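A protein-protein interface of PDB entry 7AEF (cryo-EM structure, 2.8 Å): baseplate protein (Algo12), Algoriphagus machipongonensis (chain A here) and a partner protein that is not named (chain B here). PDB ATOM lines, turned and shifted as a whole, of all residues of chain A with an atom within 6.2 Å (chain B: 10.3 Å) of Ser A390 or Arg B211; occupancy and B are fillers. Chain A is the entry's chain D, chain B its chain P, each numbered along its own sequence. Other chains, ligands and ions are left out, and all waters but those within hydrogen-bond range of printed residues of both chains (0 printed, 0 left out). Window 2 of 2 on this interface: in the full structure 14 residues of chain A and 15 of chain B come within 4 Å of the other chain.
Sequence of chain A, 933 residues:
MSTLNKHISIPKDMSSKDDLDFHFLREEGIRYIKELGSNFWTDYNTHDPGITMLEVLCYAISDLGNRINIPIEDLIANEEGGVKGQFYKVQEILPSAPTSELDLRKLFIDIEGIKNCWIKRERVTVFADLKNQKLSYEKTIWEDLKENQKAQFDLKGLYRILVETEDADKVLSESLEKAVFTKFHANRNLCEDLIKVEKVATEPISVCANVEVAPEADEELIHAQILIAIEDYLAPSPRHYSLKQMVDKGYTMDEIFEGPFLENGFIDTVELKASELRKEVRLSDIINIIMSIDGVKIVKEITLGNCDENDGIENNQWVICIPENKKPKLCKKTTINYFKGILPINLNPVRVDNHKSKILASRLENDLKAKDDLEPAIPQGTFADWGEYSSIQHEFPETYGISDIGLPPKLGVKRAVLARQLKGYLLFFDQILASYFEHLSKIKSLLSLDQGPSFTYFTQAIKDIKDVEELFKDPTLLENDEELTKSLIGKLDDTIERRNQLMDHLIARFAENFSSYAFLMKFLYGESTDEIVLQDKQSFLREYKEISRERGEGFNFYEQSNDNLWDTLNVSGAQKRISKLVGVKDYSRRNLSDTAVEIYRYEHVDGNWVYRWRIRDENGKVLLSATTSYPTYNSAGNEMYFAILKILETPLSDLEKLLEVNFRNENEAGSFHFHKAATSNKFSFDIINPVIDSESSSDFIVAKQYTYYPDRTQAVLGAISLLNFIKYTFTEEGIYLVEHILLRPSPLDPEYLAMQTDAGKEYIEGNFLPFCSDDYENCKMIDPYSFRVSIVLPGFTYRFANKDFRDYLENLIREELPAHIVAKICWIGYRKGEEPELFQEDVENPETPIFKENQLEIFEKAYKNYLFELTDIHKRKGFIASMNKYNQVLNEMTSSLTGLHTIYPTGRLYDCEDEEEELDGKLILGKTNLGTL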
ATOM      1  N   TYR A  59     -19.732 -10.932 -16.899  1.00  0.00           N
ATOM      2  CA  TYR A  59     -19.366 -10.139 -15.737  1.00  0.00           C
ATOM      3  C   TYR A  59     -20.359  -9.004 -15.518  1.00  0.00           C
ATOM      4  O   TYR A  59     -20.842  -8.799 -14.400  1.00  0.00           O
ATOM      5  CB  TYR A  59     -17.937  -9.657 -15.950  1.00  0.00           C
ATOM      6  CG  TYR A  59     -17.329  -8.822 -14.903  1.00  0.00           C
ATOM      7  CD1 TYR A  59     -17.029  -9.347 -13.671  1.00  0.00           C
ATOM      8  CD2 TYR A  59     -16.982  -7.527 -15.175  1.00  0.00           C
ATOM      9  CE1 TYR A  59     -16.426  -8.591 -12.725  1.00  0.00           C
ATOM     10  CE2 TYR A  59     -16.373  -6.766 -14.235  1.00  0.00           C
ATOM     11  CZ  TYR A  59     -16.097  -7.301 -13.012  1.00  0.00           C
ATOM     12  OH  TYR A  59     -15.478  -6.537 -12.063  1.00  0.00           O
ATOM     13  N   ALA A  60     -20.708  -8.289 -16.592  1.00  0.00           N
ATOM     14  CA  ALA A  60     -21.686  -7.206 -16.524  1.00  0.00           C
ATOM     15  C   ALA A  60     -23.058  -7.680 -16.057  1.00  0.00           C
ATOM     16  O   ALA A  60     -23.741  -6.969 -15.315  1.00  0.00           O
ATOM     17  CB  ALA A  60     -21.810  -6.552 -17.887  1.00  0.00           C
ATOM     18  N   ASP A  63     -23.248  -8.023 -12.260  1.00  0.00           N
ATOM     19  CA  ASP A  63     -23.393  -6.711 -11.630  1.00  0.00           C
ATOM     20  C   ASP A  63     -24.846  -6.270 -11.606  1.00  0.00           C
ATOM     21  O   ASP A  63     -25.343  -5.805 -10.576  1.00  0.00           O
ATOM     22  CB  ASP A  63     -22.534  -5.685 -12.371  1.00  0.00           C
ATOM     23  CG  ASP A  63     -22.559  -4.295 -11.756  1.00  0.00           C
ATOM     24  OD1 ASP A  63     -22.406  -4.170 -10.555  1.00  0.00           O
ATOM     25  OD2 ASP A  63     -22.665  -3.326 -12.500  1.00  0.00           O
ATOM     26  N   LEU A  64     -25.547  -6.438 -12.723  1.00  0.00           N
ATOM     27  CA  LEU A  64     -26.948  -6.057 -12.753  1.00  0.00           C
ATOM     28  C   LEU A  64     -27.757  -6.862 -11.756  1.00  0.00           C
ATOM     29  O   LEU A  64     -28.538  -6.288 -10.992  1.00  0.00           O
ATOM     30  CB  LEU A  64     -27.531  -6.230 -14.153  1.00  0.00           C
ATOM     31  CG  LEU A  64     -29.035  -5.945 -14.338  1.00  0.00           C
ATOM     32  CD1 LEU A  64     -29.390  -4.509 -13.968  1.00  0.00           C
ATOM     33  CD2 LEU A  64     -29.409  -6.210 -15.772  1.00  0.00           C
ATOM     34  N   ARG A  67     -27.552  -5.678  -8.144  1.00  0.00           N
ATOM     35  CA  ARG A  67     -28.275  -4.495  -7.688  1.00  0.00           C
ATOM     36  C   ARG A  67     -29.749  -4.752  -7.577  1.00  0.00           C
ATOM     37  O   ARG A  67     -30.409  -4.167  -6.718  1.00  0.00           O
ATOM     38  CB  ARG A  67     -28.092  -3.303  -8.593  1.00  0.00           C
ATOM     39  CG  ARG A  67     -26.753  -2.751  -8.540  1.00  0.00           C
ATOM     40  CD  ARG A  67     -26.729  -1.502  -9.227  1.00  0.00           C
ATOM     41  NE  ARG A  67     -25.379  -1.129  -9.505  1.00  0.00           N
ATOM     42  CZ  ARG A  67     -25.052  -0.098 -10.248  1.00  0.00           C
ATOM     43  NH1 ARG A  67     -25.960   0.692 -10.741  1.00  0.00           N
ATOM     44  NH2 ARG A  67     -23.806   0.140 -10.517  1.00  0.00           N
ATOM     45  N   GLU A 388     -26.534   4.015 -11.660  1.00  0.00           N
ATOM     46  CA  GLU A 388     -25.213   4.360 -12.192  1.00  0.00           C
ATOM     47  C   GLU A 388     -24.646   3.234 -13.058  1.00  0.00           C
ATOM     48  O   GLU A 388     -24.618   2.079 -12.641  1.00  0.00           O
ATOM     49  CB  GLU A 388     -24.236   4.641 -11.054  1.00  0.00           C
ATOM     50  CG  GLU A 388     -22.903   5.195 -11.534  1.00  0.00           C
ATOM     51  CD  GLU A 388     -21.893   5.381 -10.442  1.00  0.00           C
ATOM     52  OE1 GLU A 388     -22.215   5.184  -9.279  1.00  0.00           O
ATOM     53  OE2 GLU A 388     -20.854   5.974 -10.729  1.00  0.00           O
ATOM     54  N   TYR A 389     -24.155   3.566 -14.255  1.00  0.00           N
ATOM     55  CA  TYR A 389     -23.656   2.548 -15.179  1.00  0.00           C
ATOM     56  C   TYR A 389     -22.323   2.928 -15.810  1.00  0.00           C
ATOM     57  O   TYR A 389     -22.153   4.057 -16.265  1.00  0.00           O
ATOM     58  CB  TYR A 389     -24.674   2.302 -16.290  1.00  0.00           C
ATOM     59  CG  TYR A 389     -24.209   1.368 -17.375  1.00  0.00           C
ATOM     60  CD1 TYR A 389     -24.200   0.024 -17.160  1.00  0.00           C
ATOM     61  CD2 TYR A 389     -23.790   1.841 -18.611  1.00  0.00           C
ATOM     62  CE1 TYR A 389     -23.786  -0.836 -18.117  1.00  0.00           C
ATOM     63  CE2 TYR A 389     -23.367   0.976 -19.586  1.00  0.00           C
ATOM     64  CZ  TYR A 389     -23.372  -0.363 -19.329  1.00  0.00           C
ATOM     65  OH  TYR A 389     -22.952  -1.268 -20.269  1.00  0.00           O
ATOM     66  N   SER A 390     -21.401   1.965 -15.883  1.00  0.00           N
ATOM     67  CA  SER A 390     -20.116   2.143 -16.546  1.00  0.00           C
ATOM     68  C   SER A 390     -20.020   1.253 -17.774  1.00  0.00           C
ATOM     69  O   SER A 390     -20.392   0.083 -17.720  1.00  0.00           O
ATOM     70  CB  SER A 390     -18.972   1.783 -15.622  1.00  0.00           C
ATOM     71  OG  SER A 390     -18.929   2.624 -14.505  1.00  0.00           O
ATOM     72  N   SER A 391     -19.464   1.796 -18.854  1.00  0.00           N
ATOM     73  CA  SER A 391     -19.316   1.089 -20.124  1.00  0.00           C
ATOM     74  C   SER A 391     -18.461  -0.169 -20.051  1.00  0.00           C
ATOM     75  O   SER A 391     -17.414  -0.198 -19.402  1.00  0.00           O
ATOM     76  CB  SER A 391     -18.702   2.021 -21.144  1.00  0.00           C
ATOM     77  OG  SER A 391     -18.379   1.311 -22.303  1.00  0.00           O
ATOM     78  N   ILE A 392     -18.878  -1.197 -20.795  1.00  0.00           N
ATOM     79  CA  ILE A 392     -18.150  -2.463 -20.824  1.00  0.00           C
ATOM     80  C   ILE A 392     -16.858  -2.354 -21.601  1.00  0.00           C
ATOM     81  O   ILE A 392     -16.030  -3.262 -21.572  1.00  0.00           O
ATOM     82  CB  ILE A 392     -18.990  -3.608 -21.427  1.00  0.00           C
ATOM     83  CG1 ILE A 392     -19.287  -3.347 -22.923  1.00  0.00           C
ATOM     84  CG2 ILE A 392     -20.248  -3.791 -20.607  1.00  0.00           C
ATOM     85  CD1 ILE A 392     -19.950  -4.486 -23.678  1.00  0.00           C
ATOM     86  N   GLN A 393     -16.664  -1.244 -22.290  1.00  0.00           N
ATOM     87  CA  GLN A 393     -15.474  -1.038 -23.080  1.00  0.00           C
ATOM     88  C   GLN A 393     -14.250  -0.879 -22.189  1.00  0.00           C
ATOM     89  O   GLN A 393     -13.125  -1.138 -22.623  1.00  0.00           O
ATOM     90  CB  GLN A 393     -15.727   0.152 -24.006  1.00  0.00           C
ATOM     91  CG  GLN A 393     -16.835  -0.203 -25.008  1.00  0.00           C
ATOM     92  CD  GLN A 393     -17.260   0.877 -25.966  1.00  0.00           C
ATOM     93  OE1 GLN A 393     -16.445   1.591 -26.540  1.00  0.00           O
ATOM     94  NE2 GLN A 393     -18.565   0.986 -26.158  1.00  0.00           N
ATOM     95  N   HIS A 394     -14.456  -0.568 -20.918  1.00  0.00           N
ATOM     96  CA  HIS A 394     -13.352  -0.397 -19.993  1.00  0.00           C
ATOM     97  C   HIS A 394     -12.848  -1.718 -19.451  1.00  0.00           C
ATOM     98  O   HIS A 394     -11.879  -1.737 -18.692  1.00  0.00           O
ATOM     99  CB  HIS A 394     -13.771   0.503 -18.838  1.00  0.00           C
ATOM    100  CG  HIS A 394     -13.980   1.915 -19.239  1.00  0.00           C
ATOM    101  ND1 HIS A 394     -12.939   2.728 -19.614  1.00  0.00           N
ATOM    102  CD2 HIS A 394     -15.100   2.665 -19.340  1.00  0.00           C
ATOM    103  CE1 HIS A 394     -13.405   3.919 -19.932  1.00  0.00           C
ATOM    104  NE2 HIS A 394     -14.715   3.908 -19.777  1.00  0.00           N
ATOM    105  N   GLU A 395     -13.477  -2.817 -19.830  1.00  0.00           N
ATOM    106  CA  GLU A 395     -13.079  -4.133 -19.380  1.00  0.00           C
ATOM    107  C   GLU A 395     -12.121  -4.819 -20.343  1.00  0.00           C
ATOM    108  O   GLU A 395     -11.698  -5.943 -20.077  1.00  0.00           O
ATOM    109  CB  GLU A 395     -14.313  -5.011 -19.203  1.00  0.00           C
ATOM    110  CG  GLU A 395     -15.347  -4.502 -18.213  1.00  0.00           C
ATOM    111  CD  GLU A 395     -14.857  -4.489 -16.827  1.00  0.00           C
ATOM    112  OE1 GLU A 395     -14.074  -5.359 -16.484  1.00  0.00           O
ATOM    113  OE2 GLU A 395     -15.268  -3.627 -16.061  1.00  0.00           O
ATOM    114  N   ASP A 430     -24.041  -1.970 -24.902  1.00  0.00           N
ATOM    115  CA  ASP A 430     -24.079  -1.054 -23.779  1.00  0.00           C
ATOM    116  C   ASP A 430     -25.393  -0.326 -23.710  1.00  0.00           C
ATOM    117  O   ASP A 430     -25.864  -0.050 -22.607  1.00  0.00           O
ATOM    118  CB  ASP A 430     -23.030   0.047 -23.853  1.00  0.00           C
ATOM    119  CG  ASP A 430     -21.639  -0.370 -23.551  1.00  0.00           C
ATOM    120  OD1 ASP A 430     -21.348  -0.716 -22.397  1.00  0.00           O
ATOM    121  OD2 ASP A 430     -20.812  -0.263 -24.459  1.00  0.00           O
ATOM    122  N   PHE A 437     -30.433  -0.539 -16.075  1.00  0.00           N
ATOM    123  CA  PHE A 437     -30.047   0.162 -14.859  1.00  0.00           C
ATOM    124  C   PHE A 437     -30.922   1.379 -14.642  1.00  0.00           C
ATOM    125  O   PHE A 437     -31.337   1.669 -13.514  1.00  0.00           O
ATOM    126  CB  PHE A 437     -28.574   0.535 -14.935  1.00  0.00           C
ATOM    127  CG  PHE A 437     -27.665  -0.615 -14.646  1.00  0.00           C
ATOM    128  CD1 PHE A 437     -27.075  -1.320 -15.660  1.00  0.00           C
ATOM    129  CD2 PHE A 437     -27.414  -1.001 -13.362  1.00  0.00           C
ATOM    130  CE1 PHE A 437     -26.248  -2.377 -15.397  1.00  0.00           C
ATOM    131  CE2 PHE A 437     -26.583  -2.062 -13.104  1.00  0.00           C
ATOM    132  CZ  PHE A 437     -26.005  -2.739 -14.120  1.00  0.00           C
ATOM    133  N   ASP A 464     -19.136   7.874 -20.749  1.00  0.00           N
ATOM    134  CA  ASP A 464     -17.813   7.510 -20.282  1.00  0.00           C
ATOM    135  C   ASP A 464     -16.986   6.870 -21.397  1.00  0.00           C
ATOM    136  O   ASP A 464     -16.027   6.130 -21.146  1.00  0.00           O
ATOM    137  CB  ASP A 464     -17.889   6.584 -19.079  1.00  0.00           C
ATOM    138  CG  ASP A 464     -18.778   5.427 -19.307  1.00  0.00           C
ATOM    139  OD1 ASP A 464     -19.570   5.466 -20.244  1.00  0.00           O
ATOM    140  OD2 ASP A 464     -18.554   4.399 -18.666  1.00  0.00           O
ATOM    141  N   VAL B 178      -7.292   0.616  -1.199  1.00  0.00           N
ATOM    142  CA  VAL B 178      -7.389   0.549  -2.652  1.00  0.00           C
ATOM    143  C   VAL B 178      -6.420   1.548  -3.272  1.00  0.00           C
ATOM    144  O   VAL B 178      -6.468   2.747  -2.974  1.00  0.00           O
ATOM    145  CB  VAL B 178      -8.829   0.808  -3.117  1.00  0.00           C
ATOM    146  CG1 VAL B 178      -8.898   0.944  -4.622  1.00  0.00           C
ATOM    147  CG2 VAL B 178      -9.734  -0.306  -2.656  1.00  0.00           C
ATOM    148  N   GLY B 181      -5.311   1.177 -10.079  1.00  0.00           N
ATOM    149  CA  GLY B 181      -4.895   0.004 -10.813  1.00  0.00           C
ATOM    150  C   GLY B 181      -5.441  -1.291 -10.258  1.00  0.00           C
ATOM    151  O   GLY B 181      -5.227  -2.345 -10.866  1.00  0.00           O
ATOM    152  N   ASP B 182      -6.135  -1.251  -9.123  1.00  0.00           N
ATOM    153  CA  ASP B 182      -6.686  -2.447  -8.507  1.00  0.00           C
ATOM    154  C   ASP B 182      -8.064  -2.765  -9.068  1.00  0.00           C
ATOM    155  O   ASP B 182      -8.850  -1.872  -9.387  1.00  0.00           O
ATOM    156  CB  ASP B 182      -6.796  -2.276  -6.990  1.00  0.00           C
ATOM    157  CG  ASP B 182      -5.461  -2.355  -6.292  1.00  0.00           C
ATOM    158  OD1 ASP B 182      -4.481  -2.803  -6.922  1.00  0.00           O
ATOM    159  OD2 ASP B 182      -5.392  -1.972  -5.104  1.00  0.00           O
ATOM    160  N   THR B 183      -8.353  -4.058  -9.179  1.00  0.00           N
ATOM    161  CA  THR B 183      -9.687  -4.539  -9.497  1.00  0.00           C
ATOM    162  C   THR B 183     -10.105  -5.518  -8.416  1.00  0.00           C
ATOM    163  O   THR B 183      -9.263  -6.115  -7.747  1.00  0.00           O
ATOM    164  CB  THR B 183      -9.758  -5.221 -10.868  1.00  0.00           C
ATOM    165  OG1 THR B 183      -8.772  -6.251 -10.943  1.00  0.00           O
ATOM    166  CG2 THR B 183      -9.506  -4.224 -11.981  1.00  0.00           C
ATOM    167  N   LEU B 184     -11.412  -5.667  -8.238  1.00  0.00           N
ATOM    168  CA  LEU B 184     -11.919  -6.572  -7.209  1.00  0.00           C
ATOM    169  C   LEU B 184     -11.674  -8.061  -7.491  1.00  0.00           C
ATOM    170  O   LEU B 184     -11.325  -8.778  -6.540  1.00  0.00           O
ATOM    171  CB  LEU B 184     -13.406  -6.292  -6.946  1.00  0.00           C
ATOM    172  CG  LEU B 184     -13.992  -6.942  -5.691  1.00  0.00           C
ATOM    173  CD1 LEU B 184     -13.430  -6.311  -4.445  1.00  0.00           C
ATOM    174  CD2 LEU B 184     -15.495  -6.888  -5.675  1.00  0.00           C
ATOM    175  N   PRO B 185     -11.820  -8.603  -8.720  1.00  0.00           N
ATOM    176  CA  PRO B 185     -11.510 -10.036  -8.882  1.00  0.00           C
ATOM    177  C   PRO B 185     -10.027 -10.381  -8.831  1.00  0.00           C
ATOM    178  O   PRO B 185      -9.694 -11.525  -8.504  1.00  0.00           O
ATOM    179  CB  PRO B 185     -12.118 -10.372 -10.249  1.00  0.00           C
ATOM    180  CG  PRO B 185     -13.136  -9.372 -10.451  1.00  0.00           C
ATOM    181  CD  PRO B 185     -12.538  -8.135  -9.926  1.00  0.00           C
ATOM    182  N   MET B 187      -7.817  -8.871  -6.734  1.00  0.00           N
ATOM    183  CA  MET B 187      -7.456  -8.847  -5.318  1.00  0.00           C
ATOM    184  C   MET B 187      -8.012 -10.051  -4.576  1.00  0.00           C
ATOM    185  O   MET B 187      -7.399 -10.531  -3.618  1.00  0.00           O
ATOM    186  CB  MET B 187      -7.956  -7.560  -4.666  1.00  0.00           C
ATOM    187  CG  MET B 187      -7.181  -6.318  -5.035  1.00  0.00           C
ATOM    188  SD  MET B 187      -7.534  -4.934  -3.942  1.00  0.00           S
ATOM    189  CE  MET B 187      -9.258  -4.644  -4.297  1.00  0.00           C
ATOM    190  N   TYR B 198     -15.779 -12.719  -5.354  1.00  0.00           N
ATOM    191  CA  TYR B 198     -15.827 -11.259  -5.442  1.00  0.00           C
ATOM    192  C   TYR B 198     -17.199 -10.687  -5.092  1.00  0.00           C
ATOM    193  O   TYR B 198     -17.286  -9.539  -4.648  1.00  0.00           O
ATOM    194  CB  TYR B 198     -15.399 -10.798  -6.847  1.00  0.00           C
ATOM    195  CG  TYR B 198     -16.359 -11.153  -7.961  1.00  0.00           C
ATOM    196  CD1 TYR B 198     -16.330 -12.406  -8.553  1.00  0.00           C
ATOM    197  CD2 TYR B 198     -17.287 -10.231  -8.433  1.00  0.00           C
ATOM    198  CE1 TYR B 198     -17.202 -12.737  -9.561  1.00  0.00           C
ATOM    199  CE2 TYR B 198     -18.169 -10.558  -9.433  1.00  0.00           C
ATOM    200  CZ  TYR B 198     -18.118 -11.812  -9.999  1.00  0.00           C
ATOM    201  OH  TYR B 198     -18.985 -12.147 -11.003  1.00  0.00           O
ATOM    202  N   LEU B 199     -18.275 -11.446  -5.286  1.00  0.00           N
ATOM    203  CA  LEU B 199     -19.588 -10.931  -4.914  1.00  0.00           C
ATOM    204  C   LEU B 199     -19.857 -11.038  -3.422  1.00  0.00           C
ATOM    205  O   LEU B 199     -20.747 -10.353  -2.915  1.00  0.00           O
ATOM    206  CB  LEU B 199     -20.701 -11.643  -5.684  1.00  0.00           C
ATOM    207  CG  LEU B 199     -21.070 -11.101  -7.067  1.00  0.00           C
ATOM    208  CD1 LEU B 199     -22.267 -11.836  -7.628  1.00  0.00           C
ATOM    209  CD2 LEU B 199     -21.343  -9.621  -7.010  1.00  0.00           C
ATOM    210  N   ALA B 202     -17.960  -7.903  -1.970  1.00  0.00           N
ATOM    211  CA  ALA B 202     -18.649  -6.652  -2.250  1.00  0.00           C
ATOM    212  C   ALA B 202     -19.877  -6.481  -1.368  1.00  0.00           C
ATOM    213  O   ALA B 202     -20.238  -5.356  -1.011  1.00  0.00           O
ATOM    214  CB  ALA B 202     -19.031  -6.585  -3.730  1.00  0.00           C
ATOM    215  N   LEU B 207     -20.778  -2.450  -1.246  1.00  0.00           N
ATOM    216  CA  LEU B 207     -20.453  -1.869  -2.538  1.00  0.00           C
ATOM    217  C   LEU B 207     -21.521  -2.206  -3.570  1.00  0.00           C
ATOM    218  O   LEU B 207     -21.946  -3.357  -3.695  1.00  0.00           O
ATOM    219  CB  LEU B 207     -19.094  -2.368  -3.028  1.00  0.00           C
ATOM    220  CG  LEU B 207     -17.890  -2.076  -2.140  1.00  0.00           C
ATOM    221  CD1 LEU B 207     -16.746  -3.010  -2.475  1.00  0.00           C
ATOM    222  CD2 LEU B 207     -17.466  -0.642  -2.307  1.00  0.00           C
ATOM    223  N   THR B 208     -21.950  -1.192  -4.314  1.00  0.00           N
ATOM    224  CA  THR B 208     -22.882  -1.410  -5.406  1.00  0.00           C
ATOM    225  C   THR B 208     -22.180  -1.294  -6.746  1.00  0.00           C
ATOM    226  O   THR B 208     -22.350  -2.149  -7.621  1.00  0.00           O
ATOM    227  CB  THR B 208     -24.054  -0.422  -5.330  1.00  0.00           C
ATOM    228  OG1 THR B 208     -23.589   0.898  -5.621  1.00  0.00           O
ATOM    229  CG2 THR B 208     -24.676  -0.443  -3.947  1.00  0.00           C
ATOM    230  N   ASN B 209     -21.372  -0.251  -6.917  1.00  0.00           N
ATOM    231  CA  ASN B 209     -20.560  -0.081  -8.118  1.00  0.00           C
ATOM    232  C   ASN B 209     -19.150  -0.613  -7.859  1.00  0.00           C
ATOM    233  O   ASN B 209     -18.178   0.129  -7.728  1.00  0.00           O
ATOM    234  CB  ASN B 209     -20.539   1.384  -8.537  1.00  0.00           C
ATOM    235  CG  ASN B 209     -20.224   1.566 -10.009  1.00  0.00           C
ATOM    236  OD1 ASN B 209     -21.009   1.186 -10.875  1.00  0.00           O
ATOM    237  ND2 ASN B 209     -19.073   2.157 -10.299  1.00  0.00           N
ATOM    238  N   PHE B 210     -19.047  -1.942  -7.800  1.00  0.00           N
ATOM    239  CA  PHE B 210     -17.756  -2.565  -7.531  1.00  0.00           C
ATOM    240  C   PHE B 210     -16.859  -2.650  -8.759  1.00  0.00           C
ATOM    241  O   PHE B 210     -15.697  -3.038  -8.620  1.00  0.00           O
ATOM    242  CB  PHE B 210     -17.940  -3.963  -6.918  1.00  0.00           C
ATOM    243  CG  PHE B 210     -18.748  -4.925  -7.761  1.00  0.00           C
ATOM    244  CD1 PHE B 210     -18.138  -5.736  -8.706  1.00  0.00           C
ATOM    245  CD2 PHE B 210     -20.111  -5.057  -7.563  1.00  0.00           C
ATOM    246  CE1 PHE B 210     -18.874  -6.612  -9.462  1.00  0.00           C
ATOM    247  CE2 PHE B 210     -20.850  -5.941  -8.311  1.00  0.00           C
ATOM    248  CZ  PHE B 210     -20.228  -6.722  -9.262  1.00  0.00           C
ATOM    249  N   ARG B 211     -17.353  -2.308  -9.946  1.00  0.00           N
ATOM    250  CA  ARG B 211     -16.528  -2.431 -11.140  1.00  0.00           C
ATOM    251  C   ARG B 211     -15.626  -1.233 -11.338  1.00  0.00           C
ATOM    252  O   ARG B 211     -14.739  -1.267 -12.198  1.00  0.00           O
ATOM    253  CB  ARG B 211     -17.410  -2.663 -12.364  1.00  0.00           C
ATOM    254  CG  ARG B 211     -17.852  -4.109 -12.496  1.00  0.00           C
ATOM    255  CD  ARG B 211     -19.034  -4.283 -13.422  1.00  0.00           C
ATOM    256  NE  ARG B 211     -18.897  -3.469 -14.620  1.00  0.00           N
ATOM    257  CZ  ARG B 211     -19.919  -2.997 -15.320  1.00  0.00           C
ATOM    258  NH1 ARG B 211     -21.158  -3.257 -14.944  1.00  0.00           N
ATOM    259  NH2 ARG B 211     -19.701  -2.260 -16.395  1.00  0.00           N
ATOM    260  N   ARG B 212     -15.823  -0.217 -10.507  1.00  0.00           N
ATOM    261  CA  ARG B 212     -14.963   0.948 -10.441  1.00  0.00           C
ATOM    262  C   ARG B 212     -14.712   1.205  -8.959  1.00  0.00           C
ATOM    263  O   ARG B 212     -15.632   1.607  -8.244  1.00  0.00           O
ATOM    264  CB  ARG B 212     -15.639   2.153 -11.091  1.00  0.00           C
ATOM    265  CG  ARG B 212     -16.079   1.930 -12.529  1.00  0.00           C
ATOM    266  CD  ARG B 212     -14.886   1.790 -13.460  1.00  0.00           C
ATOM    267  NE  ARG B 212     -14.114   3.026 -13.542  1.00  0.00           N
ATOM    268  CZ  ARG B 212     -13.058   3.196 -14.331  1.00  0.00           C
ATOM    269  NH1 ARG B 212     -12.644   2.206 -15.109  1.00  0.00           N
ATOM    270  NH2 ARG B 212     -12.415   4.355 -14.341  1.00  0.00           N
ATOM    271  N   LEU B 213     -13.491   0.983  -8.479  1.00  0.00           N
ATOM    272  CA  LEU B 213     -13.182   1.279  -7.088  1.00  0.00           C
ATOM    273  C   LEU B 213     -12.480   2.625  -6.978  1.00  0.00           C
ATOM    274  O   LEU B 213     -11.643   2.973  -7.812  1.00  0.00           O
ATOM    275  CB  LEU B 213     -12.316   0.183  -6.464  1.00  0.00           C
ATOM    276  CG  LEU B 213     -12.804  -1.259  -6.605  1.00  0.00           C
ATOM    277  CD1 LEU B 213     -11.749  -2.235  -6.118  1.00  0.00           C
ATOM    278  CD2 LEU B 213     -14.104  -1.464  -5.860  1.00  0.00           C
ATOM    279  N   LYS B 214     -12.839   3.380  -5.944  1.00  0.00           N
ATOM    280  CA  LYS B 214     -12.221   4.662  -5.645  1.00  0.00           C
ATOM    281  C   LYS B 214     -10.970   4.451  -4.806  1.00  0.00           C
ATOM    282  O   LYS B 214     -10.932   3.589  -3.926  1.00  0.00           O
ATOM    283  CB  LYS B 214     -13.200   5.578  -4.911  1.00  0.00           C
ATOM    284  CG  LYS B 214     -14.577   5.637  -5.550  1.00  0.00           C
ATOM    285  CD  LYS B 214     -14.517   6.307  -6.914  1.00  0.00           C
ATOM    286  CE  LYS B 214     -15.837   6.183  -7.664  1.00  0.00           C
ATOM    287  NZ  LYS B 214     -15.923   4.933  -8.473  1.00  0.00           N
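The guanidinium group (NH1) of Arg B211 is in salt-bridge range of the side-chain carboxylate (OD2) of Asp A63.
The guanidinium group (NH2) of Arg A67 is in hydrogen-bond range of the side-chain amide oxygen (OD1) of Asn B209, at 3.0 Å.
The backbone carbonyl oxygen (O) of Ser A390 sits at hydrogen-bond distance from the guanidinium group (NH2) of Arg B211, 2.8 Å away.
OE2 of Glu A395 lies within salt-bridge range of NE of Arg B211, at 3.9 Å.
NH1 of Arg A67 is in hydrogen-bond range of O of Glu A388, 2.7 Å away.
NZ of Lys B214 is in hydrogen-bond range of O of Arg B212 (3.3 Å).
CD of Pro B185 touches OH of Tyr A59 (3.97 Å).
Arg B211 touches Tyr A59 (CG to OH, 3.4 Å).
Asp A63 touches Thr B208.
CE2 of Phe B210 touches OD1 of Asp A63 (3.3 Å).
Arg A67 touches Thr B208 (NE to O, 3.7 Å).
Arg B212 touches Ser A390 (CG to OG, 3.5 Å).
No residue of chain B comes within 4 Å of Ala A60.
No residue of chain B comes within 4 Å of Tyr A389.
Ser A390 touches just these residues of chain B: Arg B211 (2.8 Å) and Arg B212 (3.5 Å).
No residue of chain B comes within 4 Å of Ser A391.
Of the printed residues of chain A, Thr B208 touches Asp A63 (3.6 Å) and Arg A67 (3.7 Å).
Arg B211 touches just these residues of chain A: Tyr A59 (3.4 Å), Asp A63 (2.9 Å), Ser A390 (2.8 Å) and Glu A395 (3.9 Å).
Of the printed residues of chain A, Arg B212 touches Ser A390 (3.5 Å).
The nearest residue of chain B that does not touch Ser A390 is Asn B209 (4.2 Å).
The nearest printed residue of chain A that does not touch Arg B211 is Ala A60 (4.3 Å).
Among the printed residues, 10 pairs touch across the chains.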
